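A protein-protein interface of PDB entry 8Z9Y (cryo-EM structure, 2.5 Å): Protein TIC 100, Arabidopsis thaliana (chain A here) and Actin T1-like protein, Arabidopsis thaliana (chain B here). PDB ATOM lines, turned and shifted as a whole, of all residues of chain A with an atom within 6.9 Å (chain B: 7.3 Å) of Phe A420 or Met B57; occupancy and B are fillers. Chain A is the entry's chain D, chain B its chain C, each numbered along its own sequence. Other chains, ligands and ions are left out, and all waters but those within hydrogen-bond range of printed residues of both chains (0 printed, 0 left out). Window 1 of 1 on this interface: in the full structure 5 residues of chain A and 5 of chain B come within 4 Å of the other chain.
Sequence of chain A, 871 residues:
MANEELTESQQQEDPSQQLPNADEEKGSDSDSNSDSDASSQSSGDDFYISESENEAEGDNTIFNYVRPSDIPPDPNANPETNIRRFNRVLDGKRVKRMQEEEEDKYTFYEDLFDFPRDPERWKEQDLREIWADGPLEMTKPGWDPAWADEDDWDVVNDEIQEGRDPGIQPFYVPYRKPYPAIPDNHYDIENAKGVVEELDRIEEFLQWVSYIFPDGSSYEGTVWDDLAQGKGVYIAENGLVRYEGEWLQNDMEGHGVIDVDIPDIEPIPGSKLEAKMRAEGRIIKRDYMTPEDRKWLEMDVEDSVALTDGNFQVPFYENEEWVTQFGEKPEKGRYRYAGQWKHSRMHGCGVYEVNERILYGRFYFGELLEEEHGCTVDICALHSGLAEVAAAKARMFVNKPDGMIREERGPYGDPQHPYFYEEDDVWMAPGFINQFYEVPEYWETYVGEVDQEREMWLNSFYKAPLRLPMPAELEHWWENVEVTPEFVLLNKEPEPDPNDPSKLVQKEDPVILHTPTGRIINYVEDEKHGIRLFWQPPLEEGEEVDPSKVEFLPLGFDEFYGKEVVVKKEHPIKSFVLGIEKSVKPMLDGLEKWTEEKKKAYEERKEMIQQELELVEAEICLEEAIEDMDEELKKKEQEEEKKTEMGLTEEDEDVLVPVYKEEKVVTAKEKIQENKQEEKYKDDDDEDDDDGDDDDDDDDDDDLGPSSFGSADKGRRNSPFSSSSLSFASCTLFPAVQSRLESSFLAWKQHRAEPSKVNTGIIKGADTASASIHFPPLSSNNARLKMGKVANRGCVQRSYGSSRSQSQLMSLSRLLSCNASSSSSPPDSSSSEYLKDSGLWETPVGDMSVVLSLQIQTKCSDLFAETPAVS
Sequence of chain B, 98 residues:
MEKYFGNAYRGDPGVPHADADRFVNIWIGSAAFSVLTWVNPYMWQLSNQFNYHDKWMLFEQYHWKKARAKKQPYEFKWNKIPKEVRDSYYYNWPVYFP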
ATOM      1  N   PRO A 415     -18.685   5.880  -9.873  1.00  0.00           N
ATOM      2  CA  PRO A 415     -19.837   6.617  -9.326  1.00  0.00           C
ATOM      3  C   PRO A 415     -20.226   6.207  -7.913  1.00  0.00           C
ATOM      4  O   PRO A 415     -20.245   7.049  -7.009  1.00  0.00           O
ATOM      5  CB  PRO A 415     -20.963   6.300 -10.323  1.00  0.00           C
ATOM      6  CG  PRO A 415     -20.448   5.184 -11.184  1.00  0.00           C
ATOM      7  CD  PRO A 415     -18.970   5.305 -11.195  1.00  0.00           C
ATOM      8  N   HIS A 417     -22.690   5.851  -6.264  1.00  0.00           N
ATOM      9  CA  HIS A 417     -23.781   6.269  -5.385  1.00  0.00           C
ATOM     10  C   HIS A 417     -25.062   5.506  -5.717  1.00  0.00           C
ATOM     11  O   HIS A 417     -25.341   5.248  -6.891  1.00  0.00           O
ATOM     12  CB  HIS A 417     -24.036   7.767  -5.505  1.00  0.00           C
ATOM     13  CG  HIS A 417     -24.994   8.294  -4.482  1.00  0.00           C
ATOM     14  ND1 HIS A 417     -26.361   8.202  -4.623  1.00  0.00           N
ATOM     15  CD2 HIS A 417     -24.779   8.909  -3.296  1.00  0.00           C
ATOM     16  CE1 HIS A 417     -26.948   8.742  -3.570  1.00  0.00           C
ATOM     17  NE2 HIS A 417     -26.011   9.179  -2.749  1.00  0.00           N
ATOM     18  N   PRO A 418     -25.844   5.141  -4.698  1.00  0.00           N
ATOM     19  CA  PRO A 418     -27.024   4.293  -4.954  1.00  0.00           C
ATOM     20  C   PRO A 418     -28.066   4.917  -5.871  1.00  0.00           C
ATOM     21  O   PRO A 418     -28.521   4.252  -6.811  1.00  0.00           O
ATOM     22  CB  PRO A 418     -27.583   4.039  -3.543  1.00  0.00           C
ATOM     23  CG  PRO A 418     -26.870   4.999  -2.639  1.00  0.00           C
ATOM     24  CD  PRO A 418     -25.544   5.240  -3.262  1.00  0.00           C
ATOM     25  N   TYR A 419     -28.473   6.170  -5.634  1.00  0.00           N
ATOM     26  CA  TYR A 419     -29.571   6.708  -6.430  1.00  0.00           C
ATOM     27  C   TYR A 419     -29.361   8.151  -6.881  1.00  0.00           C
ATOM     28  O   TYR A 419     -30.346   8.849  -7.152  1.00  0.00           O
ATOM     29  CB  TYR A 419     -30.902   6.609  -5.668  1.00  0.00           C
ATOM     30  CG  TYR A 419     -30.896   7.193  -4.269  1.00  0.00           C
ATOM     31  CD1 TYR A 419     -30.757   8.561  -4.061  1.00  0.00           C
ATOM     32  CD2 TYR A 419     -31.051   6.379  -3.158  1.00  0.00           C
ATOM     33  CE1 TYR A 419     -30.759   9.094  -2.790  1.00  0.00           C
ATOM     34  CE2 TYR A 419     -31.054   6.904  -1.883  1.00  0.00           C
ATOM     35  CZ  TYR A 419     -30.908   8.261  -1.704  1.00  0.00           C
ATOM     36  OH  TYR A 419     -30.911   8.785  -0.433  1.00  0.00           O
ATOM     37  N   PHE A 420     -28.125   8.623  -6.977  1.00  0.00           N
ATOM     38  CA  PHE A 420     -27.845   9.970  -7.470  1.00  0.00           C
ATOM     39  C   PHE A 420     -27.111   9.834  -8.800  1.00  0.00           C
ATOM     40  O   PHE A 420     -25.883   9.752  -8.848  1.00  0.00           O
ATOM     41  CB  PHE A 420     -27.043  10.782  -6.459  1.00  0.00           C
ATOM     42  CG  PHE A 420     -27.896  11.567  -5.504  1.00  0.00           C
ATOM     43  CD1 PHE A 420     -29.228  11.812  -5.789  1.00  0.00           C
ATOM     44  CD2 PHE A 420     -27.368  12.063  -4.325  1.00  0.00           C
ATOM     45  CE1 PHE A 420     -30.017  12.533  -4.916  1.00  0.00           C
ATOM     46  CE2 PHE A 420     -28.153  12.786  -3.449  1.00  0.00           C
ATOM     47  CZ  PHE A 420     -29.479  13.020  -3.745  1.00  0.00           C
ATOM     48  N   TYR A 421     -27.880   9.809  -9.882  1.00  0.00           N
ATOM     49  CA  TYR A 421     -27.354   9.683 -11.233  1.00  0.00           C
ATOM     50  C   TYR A 421     -27.514  11.013 -11.955  1.00  0.00           C
ATOM     51  O   TYR A 421     -28.592  11.614 -11.920  1.00  0.00           O
ATOM     52  CB  TYR A 421     -28.077   8.580 -12.009  1.00  0.00           C
ATOM     53  CG  TYR A 421     -27.801   7.171 -11.531  1.00  0.00           C
ATOM     54  CD1 TYR A 421     -28.243   6.736 -10.290  1.00  0.00           C
ATOM     55  CD2 TYR A 421     -27.108   6.273 -12.329  1.00  0.00           C
ATOM     56  CE1 TYR A 421     -27.997   5.450  -9.856  1.00  0.00           C
ATOM     57  CE2 TYR A 421     -26.857   4.985 -11.903  1.00  0.00           C
ATOM     58  CZ  TYR A 421     -27.304   4.580 -10.666  1.00  0.00           C
ATOM     59  OH  TYR A 421     -27.056   3.297 -10.238  1.00  0.00           O
ATOM     60  N   GLU A 422     -26.446  11.469 -12.602  1.00  0.00           N
ATOM     61  CA  GLU A 422     -26.542  12.662 -13.424  1.00  0.00           C
ATOM     62  C   GLU A 422     -27.427  12.392 -14.636  1.00  0.00           C
ATOM     63  O   GLU A 422     -27.671  11.245 -15.015  1.00  0.00           O
ATOM     64  CB  GLU A 422     -25.155  13.121 -13.874  1.00  0.00           C
ATOM     65  CG  GLU A 422     -24.285  13.653 -12.749  1.00  0.00           C
ATOM     66  CD  GLU A 422     -24.463  15.143 -12.533  1.00  0.00           C
ATOM     67  OE1 GLU A 422     -25.408  15.722 -13.107  1.00  0.00           O
ATOM     68  OE2 GLU A 422     -23.656  15.736 -11.786  1.00  0.00           O
ATOM     69  N   ASP A 425     -26.022  10.157 -17.015  1.00  0.00           N
ATOM     70  CA  ASP A 425     -25.587   8.879 -16.466  1.00  0.00           C
ATOM     71  C   ASP A 425     -26.750   7.968 -16.093  1.00  0.00           C
ATOM     72  O   ASP A 425     -26.522   6.903 -15.508  1.00  0.00           O
ATOM     73  CB  ASP A 425     -24.695   9.101 -15.241  1.00  0.00           C
ATOM     74  CG  ASP A 425     -23.317   9.612 -15.608  1.00  0.00           C
ATOM     75  OD1 ASP A 425     -23.165  10.186 -16.705  1.00  0.00           O
ATOM     76  OD2 ASP A 425     -22.384   9.438 -14.796  1.00  0.00           O
ATOM     77  N   ASN B  51     -32.363  13.243   4.489  1.00  0.00           N
ATOM     78  CA  ASN B  51     -31.044  12.714   4.801  1.00  0.00           C
ATOM     79  C   ASN B  51     -30.044  13.857   4.711  1.00  0.00           C
ATOM     80  O   ASN B  51     -29.981  14.553   3.691  1.00  0.00           O
ATOM     81  CB  ASN B  51     -30.661  11.582   3.845  1.00  0.00           C
ATOM     82  CG  ASN B  51     -29.429  10.824   4.301  1.00  0.00           C
ATOM     83  OD1 ASN B  51     -28.780  11.199   5.277  1.00  0.00           O
ATOM     84  ND2 ASN B  51     -29.103   9.751   3.594  1.00  0.00           N
ATOM     85  N   TYR B  52     -29.271  14.053   5.781  1.00  0.00           N
ATOM     86  CA  TYR B  52     -28.402  15.222   5.865  1.00  0.00           C
ATOM     87  C   TYR B  52     -27.320  15.192   4.793  1.00  0.00           C
ATOM     88  O   TYR B  52     -27.022  16.220   4.169  1.00  0.00           O
ATOM     89  CB  TYR B  52     -27.787  15.302   7.260  1.00  0.00           C
ATOM     90  CG  TYR B  52     -28.816  15.526   8.343  1.00  0.00           C
ATOM     91  CD1 TYR B  52     -29.328  16.792   8.590  1.00  0.00           C
ATOM     92  CD2 TYR B  52     -29.292  14.468   9.103  1.00  0.00           C
ATOM     93  CE1 TYR B  52     -30.273  16.999   9.575  1.00  0.00           C
ATOM     94  CE2 TYR B  52     -30.237  14.664  10.089  1.00  0.00           C
ATOM     95  CZ  TYR B  52     -30.724  15.932  10.321  1.00  0.00           C
ATOM     96  OH  TYR B  52     -31.666  16.132  11.302  1.00  0.00           O
ATOM     97  N   HIS B  53     -26.720  14.022   4.561  1.00  0.00           N
ATOM     98  CA  HIS B  53     -25.711  13.916   3.515  1.00  0.00           C
ATOM     99  C   HIS B  53     -26.308  14.176   2.139  1.00  0.00           C
ATOM    100  O   HIS B  53     -25.638  14.741   1.272  1.00  0.00           O
ATOM    101  CB  HIS B  53     -25.044  12.543   3.554  1.00  0.00           C
ATOM    102  CG  HIS B  53     -23.844  12.435   2.668  1.00  0.00           C
ATOM    103  ND1 HIS B  53     -22.603  12.908   3.036  1.00  0.00           N
ATOM    104  CD2 HIS B  53     -23.695  11.914   1.427  1.00  0.00           C
ATOM    105  CE1 HIS B  53     -21.741  12.681   2.061  1.00  0.00           C
ATOM    106  NE2 HIS B  53     -22.378  12.079   1.073  1.00  0.00           N
ATOM    107  N   ASP B  54     -27.563  13.774   1.921  1.00  0.00           N
ATOM    108  CA  ASP B  54     -28.224  14.078   0.656  1.00  0.00           C
ATOM    109  C   ASP B  54     -28.391  15.581   0.469  1.00  0.00           C
ATOM    110  O   ASP B  54     -28.172  16.107  -0.628  1.00  0.00           O
ATOM    111  CB  ASP B  54     -29.578  13.375   0.591  1.00  0.00           C
ATOM    112  CG  ASP B  54     -29.447  11.870   0.489  1.00  0.00           C
ATOM    113  OD1 ASP B  54     -28.346  11.349   0.761  1.00  0.00           O
ATOM    114  OD2 ASP B  54     -30.445  11.208   0.136  1.00  0.00           O
ATOM    115  N   LYS B  55     -28.785  16.287   1.532  1.00  0.00           N
ATOM    116  CA  LYS B  55     -28.900  17.739   1.455  1.00  0.00           C
ATOM    117  C   LYS B  55     -27.553  18.382   1.156  1.00  0.00           C
ATOM    118  O   LYS B  55     -27.461  19.300   0.330  1.00  0.00           O
ATOM    119  CB  LYS B  55     -29.476  18.288   2.759  1.00  0.00           C
ATOM    120  CG  LYS B  55     -30.983  18.474   2.751  1.00  0.00           C
ATOM    121  CD  LYS B  55     -31.416  19.472   3.813  1.00  0.00           C
ATOM    122  CE  LYS B  55     -30.629  20.769   3.708  1.00  0.00           C
ATOM    123  NZ  LYS B  55     -31.161  21.820   4.619  1.00  0.00           N
ATOM    124  N   TRP B  56     -26.495  17.912   1.822  1.00  0.00           N
ATOM    125  CA  TRP B  56     -25.165  18.455   1.563  1.00  0.00           C
ATOM    126  C   TRP B  56     -24.733  18.195   0.128  1.00  0.00           C
ATOM    127  O   TRP B  56     -24.150  19.070  -0.522  1.00  0.00           O
ATOM    128  CB  TRP B  56     -24.156  17.861   2.545  1.00  0.00           C
ATOM    129  CG  TRP B  56     -23.967  18.692   3.772  1.00  0.00           C
ATOM    130  CD1 TRP B  56     -24.395  18.401   5.032  1.00  0.00           C
ATOM    131  CD2 TRP B  56     -23.303  19.958   3.855  1.00  0.00           C
ATOM    132  NE1 TRP B  56     -24.038  19.405   5.897  1.00  0.00           N
ATOM    133  CE2 TRP B  56     -23.365  20.372   5.199  1.00  0.00           C
ATOM    134  CE3 TRP B  56     -22.661  20.778   2.925  1.00  0.00           C
ATOM    135  CZ2 TRP B  56     -22.811  21.572   5.634  1.00  0.00           C
ATOM    136  CZ3 TRP B  56     -22.111  21.969   3.359  1.00  0.00           C
ATOM    137  CH2 TRP B  56     -22.189  22.354   4.702  1.00  0.00           C
ATOM    138  N   MET B  57     -25.012  16.994  -0.385  1.00  0.00           N
ATOM    139  CA  MET B  57     -24.657  16.671  -1.761  1.00  0.00           C
ATOM    140  C   MET B  57     -25.408  17.553  -2.747  1.00  0.00           C
ATOM    141  O   MET B  57     -24.828  18.026  -3.729  1.00  0.00           O
ATOM    142  CB  MET B  57     -24.936  15.196  -2.042  1.00  0.00           C
ATOM    143  CG  MET B  57     -24.343  14.692  -3.346  1.00  0.00           C
ATOM    144  SD  MET B  57     -23.278  13.256  -3.116  1.00  0.00           S
ATOM    145  CE  MET B  57     -24.341  12.209  -2.128  1.00  0.00           C
ATOM    146  N   LEU B  58     -26.699  17.789  -2.504  1.00  0.00           N
ATOM    147  CA  LEU B  58     -27.467  18.663  -3.386  1.00  0.00           C
ATOM    148  C   LEU B  58     -26.925  20.088  -3.363  1.00  0.00           C
ATOM    149  O   LEU B  58     -26.778  20.725  -4.415  1.00  0.00           O
ATOM    150  CB  LEU B  58     -28.941  18.645  -2.986  1.00  0.00           C
ATOM    151  CG  LEU B  58     -29.775  17.481  -3.523  1.00  0.00           C
ATOM    152  CD1 LEU B  58     -31.164  17.496  -2.914  1.00  0.00           C
ATOM    153  CD2 LEU B  58     -29.853  17.542  -5.035  1.00  0.00           C
ATOM    154  N   PHE B  59     -26.624  20.600  -2.167  1.00  0.00           N
ATOM    155  CA  PHE B  59     -26.064  21.941  -2.036  1.00  0.00           C
ATOM    156  C   PHE B  59     -24.750  22.060  -2.800  1.00  0.00           C
ATOM    157  O   PHE B  59     -24.553  22.996  -3.592  1.00  0.00           O
ATOM    158  CB  PHE B  59     -25.863  22.248  -0.550  1.00  0.00           C
ATOM    159  CG  PHE B  59     -25.324  23.619  -0.263  1.00  0.00           C
ATOM    160  CD1 PHE B  59     -26.170  24.708  -0.183  1.00  0.00           C
ATOM    161  CD2 PHE B  59     -23.971  23.810  -0.040  1.00  0.00           C
ATOM    162  CE1 PHE B  59     -25.678  25.965   0.098  1.00  0.00           C
ATOM    163  CE2 PHE B  59     -23.472  25.066   0.237  1.00  0.00           C
ATOM    164  CZ  PHE B  59     -24.327  26.144   0.308  1.00  0.00           C
ATOM    165  N   GLU B  60     -23.844  21.104  -2.581  1.00  0.00           N
ATOM    166  CA  GLU B  60     -22.548  21.140  -3.247  1.00  0.00           C
ATOM    167  C   GLU B  60     -22.697  21.011  -4.754  1.00  0.00           C
ATOM    168  O   GLU B  60     -22.004  21.699  -5.506  1.00  0.00           O
ATOM    169  CB  GLU B  60     -21.642  20.038  -2.699  1.00  0.00           C
ATOM    170  CG  GLU B  60     -21.295  20.186  -1.225  1.00  0.00           C
ATOM    171  CD  GLU B  60     -20.493  21.439  -0.925  1.00  0.00           C
ATOM    172  OE1 GLU B  60     -19.853  21.983  -1.850  1.00  0.00           O
ATOM    173  OE2 GLU B  60     -20.504  21.884   0.242  1.00  0.00           O
ATOM    174  N   GLN B  61     -23.596  20.140  -5.216  1.00  0.00           N
ATOM    175  CA  GLN B  61     -23.791  19.966  -6.650  1.00  0.00           C
ATOM    176  C   GLN B  61     -24.294  21.249  -7.294  1.00  0.00           C
ATOM    177  O   GLN B  61     -23.778  21.680  -8.334  1.00  0.00           O
ATOM    178  CB  GLN B  61     -24.766  18.818  -6.911  1.00  0.00           C
ATOM    179  CG  GLN B  61     -24.679  18.238  -8.310  1.00  0.00           C
ATOM    180  CD  GLN B  61     -26.024  18.190  -9.005  1.00  0.00           C
ATOM    181  OE1 GLN B  61     -26.975  18.849  -8.587  1.00  0.00           O
ATOM    182  NE2 GLN B  61     -26.110  17.409 -10.074  1.00  0.00           N
ATOM    183  N   TYR B  62     -25.300  21.883  -6.684  1.00  0.00           N
ATOM    184  CA  TYR B  62     -25.842  23.108  -7.260  1.00  0.00           C
ATOM    185  C   TYR B  62     -24.787  24.204  -7.311  1.00  0.00           C
ATOM    186  O   TYR B  62     -24.610  24.863  -8.343  1.00  0.00           O
ATOM    187  CB  TYR B  62     -27.058  23.583  -6.468  1.00  0.00           C
ATOM    188  CG  TYR B  62     -27.359  25.043  -6.698  1.00  0.00           C
ATOM    189  CD1 TYR B  62     -27.809  25.491  -7.931  1.00  0.00           C
ATOM    190  CD2 TYR B  62     -27.175  25.979  -5.690  1.00  0.00           C
ATOM    191  CE1 TYR B  62     -28.076  26.825  -8.152  1.00  0.00           C
ATOM    192  CE2 TYR B  62     -27.441  27.316  -5.900  1.00  0.00           C
ATOM    193  CZ  TYR B  62     -27.888  27.733  -7.133  1.00  0.00           C
ATOM    194  OH  TYR B  62     -28.158  29.064  -7.350  1.00  0.00           O
ATOM    195  N   HIS B  63     -24.066  24.411  -6.206  1.00  0.00           N
ATOM    196  CA  HIS B  63     -23.089  25.494  -6.197  1.00  0.00           C
ATOM    197  C   HIS B  63     -21.895  25.190  -7.093  1.00  0.00           C
ATOM    198  O   HIS B  63     -21.343  26.105  -7.712  1.00  0.00           O
ATOM    199  CB  HIS B  63     -22.647  25.793  -4.768  1.00  0.00           C
ATOM    200  CG  HIS B  63     -23.625  26.635  -4.012  1.00  0.00           C
ATOM    201  ND1 HIS B  63     -23.896  27.942  -4.352  1.00  0.00           N
ATOM    202  CD2 HIS B  63     -24.418  26.349  -2.954  1.00  0.00           C
ATOM    203  CE1 HIS B  63     -24.802  28.432  -3.525  1.00  0.00           C
ATOM    204  NE2 HIS B  63     -25.135  27.484  -2.667  1.00  0.00           N
ATOM    205  N   TRP B  78     -18.274  21.393   2.585  1.00  0.00           N
ATOM    206  CA  TRP B  78     -18.271  20.216   3.446  1.00  0.00           C
ATOM    207  C   TRP B  78     -16.862  19.861   3.902  1.00  0.00           C
ATOM    208  O   TRP B  78     -16.679  19.357   5.015  1.00  0.00           O
ATOM    209  CB  TRP B  78     -18.916  19.037   2.714  1.00  0.00           C
ATOM    210  CG  TRP B  78     -18.714  17.704   3.374  1.00  0.00           C
ATOM    211  CD1 TRP B  78     -17.642  16.871   3.233  1.00  0.00           C
ATOM    212  CD2 TRP B  78     -19.616  17.046   4.270  1.00  0.00           C
ATOM    213  NE1 TRP B  78     -17.819  15.740   3.990  1.00  0.00           N
ATOM    214  CE2 TRP B  78     -19.023  15.823   4.637  1.00  0.00           C
ATOM    215  CE3 TRP B  78     -20.867  17.375   4.801  1.00  0.00           C
ATOM    216  CZ2 TRP B  78     -19.637  14.928   5.508  1.00  0.00           C
ATOM    217  CZ3 TRP B  78     -21.474  16.484   5.665  1.00  0.00           C
ATOM    218  CH2 TRP B  78     -20.860  15.276   6.011  1.00  0.00           C
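The side-chain carboxylate (OD2) of Asp B54 lies within hydrogen-bond range of the side-chain hydroxyl (OH) of Tyr A419, at 2.5 Å. NE2 of Gln B61 is in hydrogen-bond range of OE2 of Glu A422, at 3.4 Å.
Of the printed residues of chain B, Phe A420 touches Met B57. Of the printed residues of chain B, Glu A422 touches Gln B61. Of the printed residues of chain A, Asp B54 touches Tyr A419 (2.5 Å). Printed residues of chain A within 4 Å of Met B57: His A417 and Phe A420. Glu B60 touches none of the printed residues of chain A. Of the printed residues of chain A, Gln B61 touches Glu A422. The nearest printed residue of chain A that does not touch Met B57 is Pro A418 (7.2 Å). The nearest printed residue of chain A that does not touch Asp B54 is Phe A420 (4.2 Å).
The side-chain amide nitrogen (ND2) of Asn B51 sits at hydrogen-bond distance from the side-chain carboxylate (OD1) of Asp B54, at 3.3 Å. The backbone NH of Tyr A419 is in hydrogen-bond range of a ring nitrogen (ND1) of His A417, at 3.1 Å. A ring nitrogen (ND1) of His A417 is in hydrogen-bond range of the backbone NH (N) of Phe A420, at 3.0 Å.
CE of Met B57 touches NE2 of His A417, 3.5 Å away. Met B57 touches Phe A420.
Hydrophobic or aromatic side chains of chain A within 4 Å of the printed part of chain B: His A417, Tyr A419 and Phe A420. Along chain A the printed residues that touch a printed residue of chain B span positions 417 to 422. Of the 14 printed residues of chain B, 3 touch a printed residue of chain A. Hydrophobic or aromatic side chains of chain B that line the printed part of chain A: Met B57. Among the printed residues, no Asp or Glu carboxylate lies within 4 Å of a Lys or Arg side-chain nitrogen of the other chain.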
